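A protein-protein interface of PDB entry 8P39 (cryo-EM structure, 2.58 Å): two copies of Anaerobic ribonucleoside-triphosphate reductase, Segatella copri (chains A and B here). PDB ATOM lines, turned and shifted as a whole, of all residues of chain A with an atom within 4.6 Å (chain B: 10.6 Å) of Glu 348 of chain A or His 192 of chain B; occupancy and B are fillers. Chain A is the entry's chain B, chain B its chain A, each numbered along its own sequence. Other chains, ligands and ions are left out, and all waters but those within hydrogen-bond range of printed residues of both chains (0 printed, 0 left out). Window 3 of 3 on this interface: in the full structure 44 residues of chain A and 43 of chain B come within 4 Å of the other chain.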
ATOM      1  N   ASN A 304     -16.508 -22.704 -19.998  1.00  0.00           N
ATOM      2  CA  ASN A 304     -15.818 -21.434 -20.178  1.00  0.00           C
ATOM      3  C   ASN A 304     -14.309 -21.583 -20.041  1.00  0.00           C
ATOM      4  O   ASN A 304     -13.556 -20.850 -20.690  1.00  0.00           O
ATOM      5  CB  ASN A 304     -16.341 -20.410 -19.172  1.00  0.00           C
ATOM      6  CG  ASN A 304     -15.695 -19.054 -19.335  1.00  0.00           C
ATOM      7  OD1 ASN A 304     -14.705 -18.743 -18.677  1.00  0.00           O
ATOM      8  ND2 ASN A 304     -16.254 -18.236 -20.217  1.00  0.00           N
ATOM      9  N   HIS A 307     -12.762 -22.960 -23.342  1.00  0.00           N
ATOM     10  CA  HIS A 307     -12.752 -21.960 -24.402  1.00  0.00           C
ATOM     11  C   HIS A 307     -11.630 -20.947 -24.221  1.00  0.00           C
ATOM     12  O   HIS A 307     -11.107 -20.425 -25.210  1.00  0.00           O
ATOM     13  CB  HIS A 307     -14.101 -21.241 -24.465  1.00  0.00           C
ATOM     14  CG  HIS A 307     -14.217 -20.267 -25.597  1.00  0.00           C
ATOM     15  ND1 HIS A 307     -13.643 -19.015 -25.566  1.00  0.00           N
ATOM     16  CD2 HIS A 307     -14.849 -20.360 -26.791  1.00  0.00           C
ATOM     17  CE1 HIS A 307     -13.911 -18.381 -26.693  1.00  0.00           C
ATOM     18  NE2 HIS A 307     -14.641 -19.175 -27.454  1.00  0.00           N
ATOM     19  N   SER A 308     -11.252 -20.653 -22.973  1.00  0.00           N
ATOM     20  CA  SER A 308     -10.171 -19.706 -22.724  1.00  0.00           C
ATOM     21  C   SER A 308      -8.821 -20.241 -23.177  1.00  0.00           C
ATOM     22  O   SER A 308      -7.876 -19.461 -23.331  1.00  0.00           O
ATOM     23  CB  SER A 308     -10.120 -19.346 -21.239  1.00  0.00           C
ATOM     24  OG  SER A 308      -9.912 -20.499 -20.441  1.00  0.00           O
ATOM     25  N   GLY A 343     -22.658 -17.682 -11.835  1.00  0.00           N
ATOM     26  CA  GLY A 343     -21.503 -17.337 -12.637  1.00  0.00           C
ATOM     27  C   GLY A 343     -20.315 -18.248 -12.373  1.00  0.00           C
ATOM     28  O   GLY A 343     -20.320 -19.104 -11.488  1.00  0.00           O
ATOM     29  N   VAL A 344     -19.278 -18.034 -13.182  1.00  0.00           N
ATOM     30  CA  VAL A 344     -18.027 -18.779 -13.114  1.00  0.00           C
ATOM     31  C   VAL A 344     -17.010 -17.953 -12.340  1.00  0.00           C
ATOM     32  O   VAL A 344     -16.996 -16.720 -12.434  1.00  0.00           O
ATOM     33  CB  VAL A 344     -17.512 -19.118 -14.528  1.00  0.00           C
ATOM     34  CG1 VAL A 344     -16.208 -19.889 -14.467  1.00  0.00           C
ATOM     35  CG2 VAL A 344     -18.554 -19.909 -15.292  1.00  0.00           C
ATOM     36  N   ASN A 346     -15.118 -15.724  -9.896  1.00  0.00           N
ATOM     37  CA  ASN A 346     -15.494 -14.699  -8.929  1.00  0.00           C
ATOM     38  C   ASN A 346     -16.756 -13.968  -9.370  1.00  0.00           C
ATOM     39  O   ASN A 346     -16.765 -12.736  -9.461  1.00  0.00           O
ATOM     40  CB  ASN A 346     -14.344 -13.709  -8.733  1.00  0.00           C
ATOM     41  CG  ASN A 346     -14.429 -12.969  -7.413  1.00  0.00           C
ATOM     42  OD1 ASN A 346     -15.515 -12.731  -6.887  1.00  0.00           O
ATOM     43  ND2 ASN A 346     -13.274 -12.603  -6.869  1.00  0.00           N
ATOM     44  N   GLY A 347     -17.823 -14.716  -9.642  1.00  0.00           N
ATOM     45  CA  GLY A 347     -19.089 -14.127 -10.034  1.00  0.00           C
ATOM     46  C   GLY A 347     -19.035 -13.354 -11.336  1.00  0.00           C
ATOM     47  O   GLY A 347     -19.557 -12.239 -11.422  1.00  0.00           O
ATOM     48  N   GLU A 348     -18.407 -13.931 -12.355  1.00  0.00           N
ATOM     49  CA  GLU A 348     -18.270 -13.285 -13.651  1.00  0.00           C
ATOM     50  C   GLU A 348     -19.070 -14.042 -14.701  1.00  0.00           C
ATOM     51  O   GLU A 348     -19.356 -15.234 -14.560  1.00  0.00           O
ATOM     52  CB  GLU A 348     -16.798 -13.196 -14.072  1.00  0.00           C
ATOM     53  CG  GLU A 348     -16.182 -14.517 -14.498  1.00  0.00           C
ATOM     54  CD  GLU A 348     -14.707 -14.393 -14.821  1.00  0.00           C
ATOM     55  OE1 GLU A 348     -14.168 -13.272 -14.725  1.00  0.00           O
ATOM     56  OE2 GLU A 348     -14.086 -15.419 -15.173  1.00  0.00           O
ATOM     57  N   THR A 349     -19.434 -13.326 -15.762  1.00  0.00           N
ATOM     58  CA  THR A 349     -20.246 -13.914 -16.817  1.00  0.00           C
ATOM     59  C   THR A 349     -19.486 -15.021 -17.533  1.00  0.00           C
ATOM     60  O   THR A 349     -18.274 -14.933 -17.747  1.00  0.00           O
ATOM     61  CB  THR A 349     -20.684 -12.845 -17.819  1.00  0.00           C
ATOM     62  OG1 THR A 349     -21.402 -13.462 -18.896  1.00  0.00           O
ATOM     63  CG2 THR A 349     -19.480 -12.107 -18.385  1.00  0.00           C
ATOM     64  N   ALA A 350     -20.206 -16.077 -17.886  1.00  0.00           N
ATOM     65  CA  ALA A 350     -19.646 -17.178 -18.653  1.00  0.00           C
ATOM     66  C   ALA A 350     -19.865 -16.902 -20.133  1.00  0.00           C
ATOM     67  O   ALA A 350     -21.009 -16.813 -20.590  1.00  0.00           O
ATOM     68  CB  ALA A 350     -20.287 -18.504 -18.248  1.00  0.00           C
ATOM     69  N   ILE A 351     -18.767 -16.757 -20.874  1.00  0.00           N
ATOM     70  CA  ILE A 351     -18.867 -16.515 -22.310  1.00  0.00           C
ATOM     71  C   ILE A 351     -19.571 -17.680 -22.990  1.00  0.00           C
ATOM     72  O   ILE A 351     -20.357 -17.492 -23.927  1.00  0.00           O
ATOM     73  CB  ILE A 351     -17.468 -16.264 -22.901  1.00  0.00           C
ATOM     74  CG1 ILE A 351     -16.812 -15.064 -22.218  1.00  0.00           C
ATOM     75  CG2 ILE A 351     -17.543 -16.037 -24.397  1.00  0.00           C
ATOM     76  CD1 ILE A 351     -17.615 -13.795 -22.322  1.00  0.00           C
ATOM     77  N   ARG A 385     -27.467 -11.882 -17.837  1.00  0.00           N
ATOM     78  CA  ARG A 385     -26.338 -12.621 -18.388  1.00  0.00           C
ATOM     79  C   ARG A 385     -26.549 -12.971 -19.857  1.00  0.00           C
ATOM     80  O   ARG A 385     -25.864 -13.852 -20.386  1.00  0.00           O
ATOM     81  CB  ARG A 385     -26.069 -13.887 -17.571  1.00  0.00           C
ATOM     82  CG  ARG A 385     -24.619 -14.339 -17.600  1.00  0.00           C
ATOM     83  CD  ARG A 385     -24.362 -15.411 -16.567  1.00  0.00           C
ATOM     84  NE  ARG A 385     -24.786 -14.987 -15.240  1.00  0.00           N
ATOM     85  CZ  ARG A 385     -24.033 -14.292 -14.399  1.00  0.00           C
ATOM     86  NH1 ARG A 385     -22.804 -13.923 -14.716  1.00  0.00           N
ATOM     87  NH2 ARG A 385     -24.527 -13.958 -13.210  1.00  0.00           N
ATOM     88  N   ARG A 683     -15.923  -5.564 -18.669  1.00  0.00           N
ATOM     89  CA  ARG A 683     -15.150  -6.570 -17.954  1.00  0.00           C
ATOM     90  C   ARG A 683     -13.981  -5.930 -17.215  1.00  0.00           C
ATOM     91  O   ARG A 683     -13.641  -4.762 -17.419  1.00  0.00           O
ATOM     92  CB  ARG A 683     -14.636  -7.649 -18.912  1.00  0.00           C
ATOM     93  CG  ARG A 683     -15.515  -8.880 -18.999  1.00  0.00           C
ATOM     94  CD  ARG A 683     -14.802 -10.005 -19.728  1.00  0.00           C
ATOM     95  NE  ARG A 683     -15.506 -11.276 -19.600  1.00  0.00           N
ATOM     96  CZ  ARG A 683     -15.313 -12.142 -18.616  1.00  0.00           C
ATOM     97  NH1 ARG A 683     -14.444 -11.905 -17.646  1.00  0.00           N
ATOM     98  NH2 ARG A 683     -16.008 -13.276 -18.604  1.00  0.00           N
ATOM     99  N   GLY A 688     -12.730  -9.234 -12.659  1.00  0.00           N
ATOM    100  CA  GLY A 688     -13.646  -9.926 -13.539  1.00  0.00           C
ATOM    101  C   GLY A 688     -15.083  -9.468 -13.439  1.00  0.00           C
ATOM    102  O   GLY A 688     -15.967 -10.141 -13.978  1.00  0.00           O
ATOM    103  N   GLU A 690     -18.619  -7.565 -13.972  1.00  0.00           N
ATOM    104  CA  GLU A 690     -19.399  -7.033 -15.079  1.00  0.00           C
ATOM    105  C   GLU A 690     -20.558  -6.212 -14.536  1.00  0.00           C
ATOM    106  O   GLU A 690     -21.214  -6.612 -13.569  1.00  0.00           O
ATOM    107  CB  GLU A 690     -19.944  -8.146 -15.982  1.00  0.00           C
ATOM    108  CG  GLU A 690     -18.895  -8.897 -16.769  1.00  0.00           C
ATOM    109  CD  GLU A 690     -18.247  -9.998 -15.968  1.00  0.00           C
ATOM    110  OE1 GLU A 690     -18.688 -10.238 -14.825  1.00  0.00           O
ATOM    111  OE2 GLU A 690     -17.298 -10.628 -16.479  1.00  0.00           O
ATOM    112  N   PHE B 188      -7.006 -20.445 -10.263  1.00  0.00           N
ATOM    113  CA  PHE B 188      -6.200 -19.915 -11.353  1.00  0.00           C
ATOM    114  C   PHE B 188      -7.117 -19.391 -12.447  1.00  0.00           C
ATOM    115  O   PHE B 188      -8.087 -20.053 -12.822  1.00  0.00           O
ATOM    116  CB  PHE B 188      -5.244 -20.975 -11.913  1.00  0.00           C
ATOM    117  CG  PHE B 188      -5.931 -22.194 -12.450  1.00  0.00           C
ATOM    118  CD1 PHE B 188      -6.355 -23.200 -11.598  1.00  0.00           C
ATOM    119  CD2 PHE B 188      -6.139 -22.343 -13.810  1.00  0.00           C
ATOM    120  CE1 PHE B 188      -6.984 -24.325 -12.093  1.00  0.00           C
ATOM    121  CE2 PHE B 188      -6.764 -23.466 -14.310  1.00  0.00           C
ATOM    122  CZ  PHE B 188      -7.188 -24.457 -13.451  1.00  0.00           C
ATOM    123  N   THR B 189      -6.796 -18.203 -12.957  1.00  0.00           N
ATOM    124  CA  THR B 189      -7.594 -17.524 -13.976  1.00  0.00           C
ATOM    125  C   THR B 189      -6.751 -17.355 -15.238  1.00  0.00           C
ATOM    126  O   THR B 189      -5.959 -16.415 -15.344  1.00  0.00           O
ATOM    127  CB  THR B 189      -8.099 -16.177 -13.464  1.00  0.00           C
ATOM    128  OG1 THR B 189      -8.312 -15.293 -14.571  1.00  0.00           O
ATOM    129  CG2 THR B 189      -7.098 -15.558 -12.502  1.00  0.00           C
ATOM    130  N   ALA B 190      -6.929 -18.262 -16.194  1.00  0.00           N
ATOM    131  CA  ALA B 190      -6.258 -18.194 -17.486  1.00  0.00           C
ATOM    132  C   ALA B 190      -7.267 -17.787 -18.549  1.00  0.00           C
ATOM    133  O   ALA B 190      -8.351 -18.374 -18.636  1.00  0.00           O
ATOM    134  CB  ALA B 190      -5.617 -19.536 -17.847  1.00  0.00           C
ATOM    135  N   GLY B 191      -6.910 -16.792 -19.352  1.00  0.00           N
ATOM    136  CA  GLY B 191      -7.844 -16.275 -20.340  1.00  0.00           C
ATOM    137  C   GLY B 191      -9.045 -15.659 -19.650  1.00  0.00           C
ATOM    138  O   GLY B 191      -8.915 -14.753 -18.818  1.00  0.00           O
ATOM    139  N   HIS B 192     -10.237 -16.141 -19.994  1.00  0.00           N
ATOM    140  CA  HIS B 192     -11.460 -15.743 -19.312  1.00  0.00           C
ATOM    141  C   HIS B 192     -12.007 -16.830 -18.397  1.00  0.00           C
ATOM    142  O   HIS B 192     -13.067 -16.636 -17.793  1.00  0.00           O
ATOM    143  CB  HIS B 192     -12.531 -15.329 -20.328  1.00  0.00           C
ATOM    144  CG  HIS B 192     -12.713 -16.304 -21.449  1.00  0.00           C
ATOM    145  ND1 HIS B 192     -12.139 -16.124 -22.689  1.00  0.00           N
ATOM    146  CD2 HIS B 192     -13.404 -17.464 -21.520  1.00  0.00           C
ATOM    147  CE1 HIS B 192     -12.468 -17.134 -23.474  1.00  0.00           C
ATOM    148  NE2 HIS B 192     -13.235 -17.961 -22.789  1.00  0.00           N
ATOM    149  N   GLY B 193     -11.313 -17.961 -18.270  1.00  0.00           N
ATOM    150  CA  GLY B 193     -11.749 -19.029 -17.389  1.00  0.00           C
ATOM    151  C   GLY B 193     -11.154 -18.870 -16.006  1.00  0.00           C
ATOM    152  O   GLY B 193      -9.941 -18.694 -15.857  1.00  0.00           O
ATOM    153  N   SER B 194     -12.011 -18.939 -14.990  1.00  0.00           N
ATOM    154  CA  SER B 194     -11.611 -18.722 -13.609  1.00  0.00           C
ATOM    155  C   SER B 194     -12.215 -19.797 -12.717  1.00  0.00           C
ATOM    156  O   SER B 194     -13.240 -20.400 -13.050  1.00  0.00           O
ATOM    157  CB  SER B 194     -12.036 -17.334 -13.119  1.00  0.00           C
ATOM    158  OG  SER B 194     -11.594 -17.102 -11.793  1.00  0.00           O
ATOM    159  N   SER B 195     -11.569 -20.029 -11.576  1.00  0.00           N
ATOM    160  CA  SER B 195     -12.013 -21.033 -10.619  1.00  0.00           C
ATOM    161  C   SER B 195     -11.734 -20.544  -9.204  1.00  0.00           C
ATOM    162  O   SER B 195     -10.948 -19.618  -8.986  1.00  0.00           O
ATOM    163  CB  SER B 195     -11.332 -22.386 -10.855  1.00  0.00           C
ATOM    164  OG  SER B 195     -11.666 -22.909 -12.130  1.00  0.00           O
ATOM    165  N   ARG B 196     -12.396 -21.180  -8.240  1.00  0.00           N
ATOM    166  CA  ARG B 196     -12.278 -20.858  -6.827  1.00  0.00           C
ATOM    167  C   ARG B 196     -11.382 -21.862  -6.117  1.00  0.00           C
ATOM    168  O   ARG B 196     -11.147 -22.965  -6.617  1.00  0.00           O
ATOM    169  CB  ARG B 196     -13.662 -20.840  -6.168  1.00  0.00           C
ATOM    170  CG  ARG B 196     -14.572 -19.736  -6.666  1.00  0.00           C
ATOM    171  CD  ARG B 196     -15.718 -19.491  -5.696  1.00  0.00           C
ATOM    172  NE  ARG B 196     -16.697 -18.553  -6.233  1.00  0.00           N
ATOM    173  CZ  ARG B 196     -17.827 -18.912  -6.825  1.00  0.00           C
ATOM    174  NH1 ARG B 196     -18.166 -20.184  -6.954  1.00  0.00           N
ATOM    175  NH2 ARG B 196     -18.638 -17.970  -7.298  1.00  0.00           N
ATOM    176  N   ILE B 210      -6.710 -29.500 -14.859  1.00  0.00           N
ATOM    177  CA  ILE B 210      -6.795 -28.314 -15.706  1.00  0.00           C
ATOM    178  C   ILE B 210      -5.479 -27.547 -15.695  1.00  0.00           C
ATOM    179  O   ILE B 210      -5.077 -26.966 -16.710  1.00  0.00           O
ATOM    180  CB  ILE B 210      -7.975 -27.432 -15.266  1.00  0.00           C
ATOM    181  CG1 ILE B 210      -9.244 -28.275 -15.140  1.00  0.00           C
ATOM    182  CG2 ILE B 210      -8.198 -26.305 -16.261  1.00  0.00           C
ATOM    183  CD1 ILE B 210     -10.421 -27.521 -14.576  1.00  0.00           C
ATOM    184  N   THR B 214      -3.826 -26.298 -19.455  1.00  0.00           N
ATOM    185  CA  THR B 214      -3.628 -24.959 -19.997  1.00  0.00           C
ATOM    186  C   THR B 214      -2.162 -24.698 -20.322  1.00  0.00           C
ATOM    187  O   THR B 214      -1.847 -24.085 -21.349  1.00  0.00           O
ATOM    188  CB  THR B 214      -4.153 -23.917 -19.010  1.00  0.00           C
ATOM    189  OG1 THR B 214      -5.524 -24.198 -18.704  1.00  0.00           O
ATOM    190  CG2 THR B 214      -4.051 -22.520 -19.599  1.00  0.00           C
ATOM    191  N   GLU B 218       1.046 -23.778 -24.074  1.00  0.00           N
ATOM    192  CA  GLU B 218       2.022 -22.702 -24.034  1.00  0.00           C
ATOM    193  C   GLU B 218       3.459 -23.194 -24.158  1.00  0.00           C
ATOM    194  O   GLU B 218       4.378 -22.371 -24.186  1.00  0.00           O
ATOM    195  CB  GLU B 218       1.856 -21.905 -22.740  1.00  0.00           C
ATOM    196  CG  GLU B 218       0.432 -21.443 -22.495  1.00  0.00           C
ATOM    197  CD  GLU B 218       0.204 -20.966 -21.080  1.00  0.00           C
ATOM    198  OE1 GLU B 218       1.186 -20.868 -20.318  1.00  0.00           O
ATOM    199  OE2 GLU B 218      -0.960 -20.694 -20.725  1.00  0.00           O
ATOM    200  N   PRO B 498       0.120 -17.191 -21.022  1.00  0.00           N
ATOM    201  CA  PRO B 498      -0.743 -16.669 -19.950  1.00  0.00           C
ATOM    202  C   PRO B 498      -0.621 -17.403 -18.624  1.00  0.00           C
ATOM    203  O   PRO B 498      -0.754 -16.768 -17.572  1.00  0.00           O
ATOM    204  CB  PRO B 498      -2.154 -16.803 -20.544  1.00  0.00           C
ATOM    205  CG  PRO B 498      -2.027 -17.812 -21.629  1.00  0.00           C
ATOM    206  CD  PRO B 498      -0.653 -17.658 -22.185  1.00  0.00           C
ATOM    207  N   LEU B 499      -0.372 -18.713 -18.627  1.00  0.00           N
ATOM    208  CA  LEU B 499      -0.309 -19.475 -17.383  1.00  0.00           C
ATOM    209  C   LEU B 499       1.105 -19.882 -16.991  1.00  0.00           C
ATOM    210  O   LEU B 499       1.443 -19.843 -15.804  1.00  0.00           O
ATOM    211  CB  LEU B 499      -1.180 -20.732 -17.476  1.00  0.00           C
ATOM    212  CG  LEU B 499      -1.290 -21.523 -16.170  1.00  0.00           C
ATOM    213  CD1 LEU B 499      -2.118 -20.759 -15.154  1.00  0.00           C
ATOM    214  CD2 LEU B 499      -1.861 -22.910 -16.401  1.00  0.00           C
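The side-chain carboxylate (OE2) of Glu 348 of chain A lies close to the backbone carbonyl oxygen (O) of His 192 of chain B (3.1 Å). A ring nitrogen (NE2) of His 192 of chain B is in hydrogen-bond range of the backbone NH (N) of Ser 308 of chain A (3.3 Å). A ring nitrogen (ND1) of His 307 of chain A sits at hydrogen-bond distance from a ring nitrogen (NE2) of His 192 of chain B (3.0 Å). O of His 192 of chain B sits close to OD1 of Asn 304 of chain A, at 2.8 Å. The side-chain hydroxyl of Ser 308 of chain A is in hydrogen-bond range of the backbone carbonyl oxygen of Ala 190 of chain B.
The side-chain carboxylate (OE1) of Glu 348 of chain A is in salt-bridge range of the guanidinium group (NH1) of Arg 683 of chain A, 3.2 Å away. The side-chain amide nitrogen (ND2) of Asn 304 of chain A lies close to the backbone NH (N) of Ile 351 of chain A (3.0 Å).
Gly 193 of chain B touches Asn 304 of chain A. Ser 308 of chain A touches Gly 191 of chain B (CB to CA, 3.9 Å). Gly 193 of chain B touches Ser 308 of chain A. Val 344 of chain A touches Ser 194 of chain B (CG1 to O, 3.3 Å). Glu 348 of chain A touches Ser 194 of chain B (OE2 to CB, 3.5 Å).
Asn 304 of chain A touches just these residues of chain B: His 192 (2.8 Å) and Gly 193 (3.2 Å). Ser 308 of chain A touches four residues of chain B. No residue of chain B comes within 4 Å of Gly 343 of chain A. Val 344 of chain A touches just one residue of chain B: Ser 194 (3.3 Å). Glu 348 of chain A touches just these residues of chain B: His 192 and Ser 194. No residue of chain B comes within 4 Å of Thr 349 of chain A. No residue of chain B comes within 4 Å of Ala 350 of chain A. Of the printed residues of chain A, Ala 190 of chain B touches Ser 308 (3.2 Å). Of the printed residues of chain A, Gly 191 of chain B touches Ser 308. Of chain A, only Asn 304, His 307, Ser 308 and Glu 348 come within 4 Å of His 192 of chain B. Of the printed residues of chain A, Gly 193 of chain B touches Asn 304 and Ser 308. Printed residues of chain A within 4 Å of Ser 194 of chain B: Val 344 (3.3 Å) and Glu 348 (3.5 Å). The nearest residue of chain B that does not touch Glu 348 of chain A is Gly 193 of chain B (4.6 Å). The nearest residue of chain A that does not touch His 192 of chain B is Ile 351 of chain A (4.2 Å). The nearest printed residue of chain A that does not touch Ala 190 of chain B is Asn 304 of chain A (6.1 Å).
Printed residues of chain B that touch a printed residue of chain A: Ala 190, Gly 191, His 192, Gly 193 and Ser 194. Hydrophobic or aromatic side chains of chain B within 4 Å of the printed part of chain A: His 192. Along chain A the printed residues that touch a printed residue of chain B span positions 304 to 348. Among the printed residues, 10 pairs touch across the chains. Among the printed residues, no Asp or Glu carboxylate lies within 4 Å of a Lys or Arg side-chain nitrogen of the other chain.
No position is printed for both chains. Of the 10 pairs that touch across the chains among the printed residues, none has its exchanged pair printed and touching as well.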
